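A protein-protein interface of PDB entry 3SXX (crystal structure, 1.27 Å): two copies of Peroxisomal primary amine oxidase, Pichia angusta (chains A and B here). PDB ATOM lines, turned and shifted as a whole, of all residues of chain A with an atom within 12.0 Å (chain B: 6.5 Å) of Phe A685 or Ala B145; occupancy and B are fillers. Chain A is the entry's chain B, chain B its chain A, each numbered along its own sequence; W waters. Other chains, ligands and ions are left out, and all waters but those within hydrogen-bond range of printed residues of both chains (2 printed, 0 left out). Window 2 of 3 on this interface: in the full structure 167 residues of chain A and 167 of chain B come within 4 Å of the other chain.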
ATOM      1  N   LYS A 669      20.650  -1.114  30.795  1.00  0.00           N
ATOM      2  CA  LYS A 669      20.212  -0.456  32.055  1.00  0.00           C
ATOM      3  C   LYS A 669      19.332  -1.354  32.881  1.00  0.00           C
ATOM      4  O   LYS A 669      19.394  -1.314  34.114  1.00  0.00           O
ATOM      5  CB  LYS A 669      19.464   0.851  31.778  1.00  0.00           C
ATOM      6  CG  LYS A 669      20.404   2.017  31.373  1.00  0.00           C
ATOM      7  CD  LYS A 669      19.558   3.231  31.054  1.00  0.00           C
ATOM      8  CE  LYS A 669      20.366   4.486  30.702  1.00  0.00           C
ATOM      9  NZ  LYS A 669      19.583   5.672  31.205  1.00  0.00           N
ATOM     10  N   PHE A 685      21.940  17.682  35.225  1.00  0.00           N
ATOM     11  CA  PHE A 685      21.940  16.572  34.282  1.00  0.00           C
ATOM     12  C   PHE A 685      23.038  15.569  34.540  1.00  0.00           C
ATOM     13  O   PHE A 685      24.172  15.954  34.786  1.00  0.00           O
ATOM     14  CB  PHE A 685      22.080  17.093  32.854  1.00  0.00           C
ATOM     15  CG  PHE A 685      20.992  18.074  32.476  1.00  0.00           C
ATOM     16  CD1 PHE A 685      19.688  17.653  32.264  1.00  0.00           C
ATOM     17  CD2 PHE A 685      21.249  19.438  32.447  1.00  0.00           C
ATOM     18  CE1 PHE A 685      18.667  18.575  32.017  1.00  0.00           C
ATOM     19  CE2 PHE A 685      20.270  20.345  32.110  1.00  0.00           C
ATOM     20  CZ  PHE A 685      18.961  19.928  31.946  1.00  0.00           C
ATOM     21  N   GLU A 686      22.689  14.283  34.505  1.00  0.00           N
ATOM     22  CA  GLU A 686      23.665  13.191  34.644  1.00  0.00           C
ATOM     23  C   GLU A 686      24.677  13.183  33.490  1.00  0.00           C
ATOM     24  O   GLU A 686      24.365  13.510  32.339  1.00  0.00           O
ATOM     25  CB  GLU A 686      22.980  11.830  34.595  1.00  0.00           C
ATOM     26  CG  GLU A 686      22.463  11.298  35.917  1.00  0.00           C
ATOM     27  CD  GLU A 686      22.088   9.831  35.814  1.00  0.00           C
ATOM     28  OE1 GLU A 686      21.958   9.350  34.673  1.00  0.00           O
ATOM     29  OE2 GLU A 686      21.970   9.158  36.863  1.00  0.00           O
ATOM     30  N   GLY A 687      25.895  12.735  33.787  1.00  0.00           N
ATOM     31  CA  GLY A 687      26.893  12.511  32.745  1.00  0.00           C
ATOM     32  C   GLY A 687      26.762  11.151  32.095  1.00  0.00           C
ATOM     33  O   GLY A 687      25.690  10.559  32.131  1.00  0.00           O
ATOM     34  N   SER A 688      27.891  10.647  31.599  1.00  0.00           N
ATOM     35  CA  SER A 688      27.990   9.342  30.960  1.00  0.00           C
ATOM     36  C   SER A 688      27.771   8.290  32.023  1.00  0.00           C
ATOM     37  O   SER A 688      28.198   8.467  33.166  1.00  0.00           O
ATOM     38  CB  SER A 688      29.415   9.163  30.374  1.00  0.00           C
ATOM     39  OG  SER A 688      29.682  10.110  29.330  1.00  0.00           O
ATOM     40  N   CYS A 689      27.216   7.143  31.650  1.00  0.00           N
ATOM     41  CA  CYS A 689      27.010   6.093  32.635  1.00  0.00           C
ATOM     42  C   CYS A 689      28.359   5.756  33.279  1.00  0.00           C
ATOM     43  O   CYS A 689      28.454   5.527  34.500  1.00  0.00           O
ATOM     44  CB  CYS A 689      26.437   4.865  31.904  1.00  0.00           C
ATOM     45  SG  CYS A 689      26.180   3.386  32.834  1.00  0.00           S
ATOM     46  N   CYS A 690      29.407   5.689  32.445  1.00  0.00           N
ATOM     47  CA  CYS A 690      30.757   5.283  32.877  1.00  0.00           C
ATOM     48  C   CYS A 690      31.506   6.365  33.659  1.00  0.00           C
ATOM     49  O   CYS A 690      32.545   6.089  34.273  1.00  0.00           O
ATOM     50  CB  CYS A 690      31.594   4.850  31.651  1.00  0.00           C
ATOM     51  SG  CYS A 690      31.866   6.187  30.387  1.00  0.00           S
ATOM     52  N   GLY A 691      30.954   7.577  33.712  1.00  0.00           N
ATOM     53  CA  GLY A 691      31.544   8.667  34.516  1.00  0.00           C
ATOM     54  C   GLY A 691      31.196   8.540  35.986  1.00  0.00           C
ATOM     55  O   GLY A 691      30.342   7.715  36.351  1.00  0.00           O
ATOM     56  N   GLU B 126      28.881  15.076  30.887  1.00  0.00           N
ATOM     57  CA  GLU B 126      28.348  15.766  32.105  1.00  0.00           C
ATOM     58  C   GLU B 126      28.673  17.252  32.022  1.00  0.00           C
ATOM     59  O   GLU B 126      27.842  18.115  32.338  1.00  0.00           O
ATOM     60  CB  GLU B 126      28.936  15.168  33.434  1.00  0.00           C
ATOM     61  CG  GLU B 126      28.382  15.810  34.759  1.00  0.00           C
ATOM     62  CD  GLU B 126      28.932  15.180  36.088  1.00  0.00           C
ATOM     63  OE1 GLU B 126      29.981  14.466  36.112  1.00  0.00           O
ATOM     64  OE2 GLU B 126      28.286  15.420  37.141  1.00  0.00           O
ATOM     65  N   ARG B 129      26.616  18.986  29.249  1.00  0.00           N
ATOM     66  CA  ARG B 129      25.177  19.032  29.472  1.00  0.00           C
ATOM     67  C   ARG B 129      24.810  20.105  30.480  1.00  0.00           C
ATOM     68  O   ARG B 129      23.702  20.592  30.438  1.00  0.00           O
ATOM     69  CB  ARG B 129      24.628  17.686  30.016  1.00  0.00           C
ATOM     70  CG  ARG B 129      24.520  16.615  28.892  1.00  0.00           C
ATOM     71  CD  ARG B 129      24.017  15.349  29.533  1.00  0.00           C
ATOM     72  NE  ARG B 129      23.813  14.341  28.450  1.00  0.00           N
ATOM     73  CZ  ARG B 129      24.144  13.063  28.515  1.00  0.00           C
ATOM     74  NH1 ARG B 129      24.584  12.526  29.625  1.00  0.00           N
ATOM     75  NH2 ARG B 129      24.013  12.308  27.451  1.00  0.00           N
ATOM     76  N   ASN B 130      25.750  20.439  31.393  1.00  0.00           N
ATOM     77  CA  ASN B 130      25.490  21.384  32.491  1.00  0.00           C
ATOM     78  C   ASN B 130      26.040  22.750  32.243  1.00  0.00           C
ATOM     79  O   ASN B 130      25.930  23.639  33.115  1.00  0.00           O
ATOM     80  CB  ASN B 130      25.982  20.772  33.805  1.00  0.00           C
ATOM     81  CG  ASN B 130      25.072  19.607  34.189  1.00  0.00           C
ATOM     82  OD1 ASN B 130      23.922  19.831  34.598  1.00  0.00           O
ATOM     83  ND2 ASN B 130      25.523  18.382  33.995  1.00  0.00           N
ATOM     84  N   ILE B 135      24.160  24.852  26.757  1.00  0.00           N
ATOM     85  CA  ILE B 135      22.706  24.737  26.800  1.00  0.00           C
ATOM     86  C   ILE B 135      22.116  25.794  25.872  1.00  0.00           C
ATOM     87  O   ILE B 135      21.233  25.483  25.061  1.00  0.00           O
ATOM     88  CB  ILE B 135      22.187  24.883  28.211  1.00  0.00           C
ATOM     89  CG1 ILE B 135      22.666  23.723  29.114  1.00  0.00           C
ATOM     90  CG2 ILE B 135      20.643  24.987  28.219  1.00  0.00           C
ATOM     91  CD1 ILE B 135      22.559  23.949  30.627  1.00  0.00           C
ATOM     92  N   CYS B 138      22.368  24.616  22.343  1.00  0.00           N
ATOM     93  CA  CYS B 138      21.409  23.538  22.088  1.00  0.00           C
ATOM     94  C   CYS B 138      20.032  24.130  21.796  1.00  0.00           C
ATOM     95  O   CYS B 138      19.370  23.722  20.827  1.00  0.00           O
ATOM     96  CB  CYS B 138      21.348  22.548  23.230  1.00  0.00           C
ATOM     97  SG  CYS B 138      22.852  21.554  23.359  1.00  0.00           S
ATOM     98  N   VAL B 139      19.656  25.144  22.585  1.00  0.00           N
ATOM     99  CA  VAL B 139      18.354  25.797  22.374  1.00  0.00           C
ATOM    100  C   VAL B 139      18.307  26.498  21.031  1.00  0.00           C
ATOM    101  O   VAL B 139      17.319  26.338  20.257  1.00  0.00           O
ATOM    102  CB  VAL B 139      18.024  26.747  23.544  1.00  0.00           C
ATOM    103  CG1 VAL B 139      16.756  27.535  23.237  1.00  0.00           C
ATOM    104  CG2 VAL B 139      17.865  25.957  24.829  1.00  0.00           C
ATOM    105  N   ILE B 143      16.831  22.366  20.367  1.00  0.00           N
ATOM    106  CA  ILE B 143      16.618  21.391  21.444  1.00  0.00           C
ATOM    107  C   ILE B 143      16.279  22.171  22.713  1.00  0.00           C
ATOM    108  O   ILE B 143      17.050  23.009  23.142  1.00  0.00           O
ATOM    109  CB  ILE B 143      17.884  20.575  21.669  1.00  0.00           C
ATOM    110  CG1 ILE B 143      18.185  19.787  20.352  1.00  0.00           C
ATOM    111  CG2 ILE B 143      17.748  19.624  22.920  1.00  0.00           C
ATOM    112  CD1 ILE B 143      19.543  19.254  20.323  1.00  0.00           C
ATOM    113  N   PRO B 144      15.103  21.941  23.293  1.00  0.00           N
ATOM    114  CA  PRO B 144      14.757  22.764  24.497  1.00  0.00           C
ATOM    115  C   PRO B 144      15.731  22.532  25.645  1.00  0.00           C
ATOM    116  O   PRO B 144      16.292  21.419  25.821  1.00  0.00           O
ATOM    117  CB  PRO B 144      13.354  22.255  24.879  1.00  0.00           C
ATOM    118  CG  PRO B 144      12.854  21.554  23.664  1.00  0.00           C
ATOM    119  CD  PRO B 144      14.039  21.005  22.924  1.00  0.00           C
ATOM    120  N   ALA B 145      15.859  23.543  26.494  1.00  0.00           N
ATOM    121  CA  ALA B 145      16.793  23.517  27.584  1.00  0.00           C
ATOM    122  C   ALA B 145      16.584  22.409  28.575  1.00  0.00           C
ATOM    123  O   ALA B 145      17.553  21.974  29.212  1.00  0.00           O
ATOM    124  CB  ALA B 145      16.826  24.884  28.331  1.00  0.00           C
ATOM    125  N   ASN B 146      15.348  21.960  28.732  1.00  0.00           N
ATOM    126  CA  ASN B 146      15.046  20.891  29.671  1.00  0.00           C
ATOM    127  C   ASN B 146      15.226  19.497  29.058  1.00  0.00           C
ATOM    128  O   ASN B 146      14.958  18.501  29.758  1.00  0.00           O
ATOM    129  CB  ASN B 146      13.661  21.060  30.293  1.00  0.00           C
ATOM    130  CG  ASN B 146      12.517  20.939  29.268  1.00  0.00           C
ATOM    131  OD1 ASN B 146      12.712  20.989  28.067  1.00  0.00           O
ATOM    132  ND2 ASN B 146      11.300  21.007  29.777  1.00  0.00           N
ATOM    133  N   GLU B 147      15.781  19.414  27.849  1.00  0.00           N
ATOM    134  CA  GLU B 147      16.031  18.153  27.155  1.00  0.00           C
ATOM    135  C   GLU B 147      17.510  17.887  26.953  1.00  0.00           C
ATOM    136  O   GLU B 147      17.924  17.105  26.076  1.00  0.00           O
ATOM    137  CB  GLU B 147      15.273  18.086  25.852  1.00  0.00           C
ATOM    138  CG  GLU B 147      13.750  18.100  26.128  1.00  0.00           C
ATOM    139  CD  GLU B 147      12.866  17.896  24.894  1.00  0.00           C
ATOM    140  OE1 GLU B 147      13.357  17.395  23.842  1.00  0.00           O
ATOM    141  OE2 GLU B 147      11.624  18.121  25.022  1.00  0.00           O
ATOM    142  N   MET B 148      18.338  18.412  27.839  1.00  0.00           N
ATOM    143  CA  MET B 148      19.778  18.163  27.757  1.00  0.00           C
ATOM    144  C   MET B 148      20.164  16.723  27.932  1.00  0.00           C
ATOM    145  O   MET B 148      21.258  16.302  27.467  1.00  0.00           O
ATOM    146  CB  MET B 148      20.574  19.060  28.709  1.00  0.00           C
ATOM    147  CG  MET B 148      20.505  20.570  28.368  1.00  0.00           C
ATOM    148  SD  MET B 148      21.142  20.954  26.697  1.00  0.00           S
ATOM    149  CE  MET B 148      22.834  20.409  26.903  1.00  0.00           C
ATOM    150  N   HIS B 149      19.309  15.901  28.538  1.00  0.00           N
ATOM    151  CA  HIS B 149      19.647  14.468  28.631  1.00  0.00           C
ATOM    152  C   HIS B 149      19.646  13.799  27.277  1.00  0.00           C
ATOM    153  O   HIS B 149      20.131  12.677  27.157  1.00  0.00           O
ATOM    154  CB  HIS B 149      18.668  13.745  29.573  1.00  0.00           C
ATOM    155  CG  HIS B 149      17.305  13.485  28.975  1.00  0.00           C
ATOM    156  ND1 HIS B 149      16.277  14.414  29.004  1.00  0.00           N
ATOM    157  CD2 HIS B 149      16.837  12.439  28.237  1.00  0.00           C
ATOM    158  CE1 HIS B 149      15.201  13.900  28.422  1.00  0.00           C
ATOM    159  NE2 HIS B 149      15.519  12.710  27.932  1.00  0.00           N
HETATM  160  O   HOH W   1      25.729  15.456  36.939  1.00  0.00           O
HETATM  161  O   HOH W   2      29.908  12.454  31.664  1.00  0.00           O
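NH1 of Arg B129 is in hydrogen-bond range of O of Glu A686 (2.9 Å). O of Gly A687 sits at hydrogen-bond distance from NH1 of Arg B129, 3.4 Å away. The backbone carbonyl oxygen of Phe A685 lies within hydrogen-bond range of the side-chain amide nitrogen of Asn B130 (2.9 Å).
The backbone carbonyl oxygen of Glu B126 sits at hydrogen-bond distance from the side-chain amide nitrogen of Asn B130 (2.9 Å). NE of Arg B129 lies within hydrogen-bond range of O of Met B148, 3.4 Å away. The side-chain sulfur of Met B148 lies close to the side-chain sulfur of Cys B138 (3.8 Å).
Among the printed residues, pairs that only touch across the chains: Phe A685 with Arg B129, Gly A687 with Glu B126, Phe A685 with Met B148 and Phe A685 with Ala B145.
Of the printed residues of chain B, Glu A686 touches Arg B129 (2.9 Å). Of the printed residues of chain B, Gly A687 touches Glu B126 and Arg B129. Gly A691 touches none of the printed residues of chain B. Printed residues of chain A within 4 Å of Glu B126: Gly A687. No residue of chain A comes within 4 Å of Ile B135. No residue of chain A comes within 4 Å of Cys B138. No residue of chain A comes within 4 Å of Val B139. Ala B145 touches one residue of chain A. No residue of chain A comes within 4 Å of Asn B146. No residue of chain A comes within 4 Å of Glu B147. Of chain A, only Phe A685 (3.6 Å) comes within 4 Å of Met B148.
Of the 8 printed residues of chain A, 3 touch a printed residue of chain B. Printed residues of chain A that touch a printed residue of chain B: Phe A685, Glu A686 and Gly A687. Hydrophobic or aromatic side chains of chain A within 4 Å of the printed part of chain B: Phe A685. Along chain A the printed residues that touch a printed residue of chain B span positions 685 to 687. Among the printed residues, 7 pairs touch across the chains. Among the printed residues, no Asp or Glu carboxylate lies within 4 Å of a Lys or Arg side-chain nitrogen of the other chain.
No position is printed for both chains. Of the 7 pairs that touch across the chains among the printed residues, none has its exchanged pair printed and touching as well.
Water W1 bridges OE2 of Glu B126 (2.6 Å) and O of Phe A685 (2.7 Å). Water W2 lies within hydrogen-bond range of the backbone NH of Ser A688 (2.7 Å) and the backbone NH of Glu B126 (2.9 Å).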
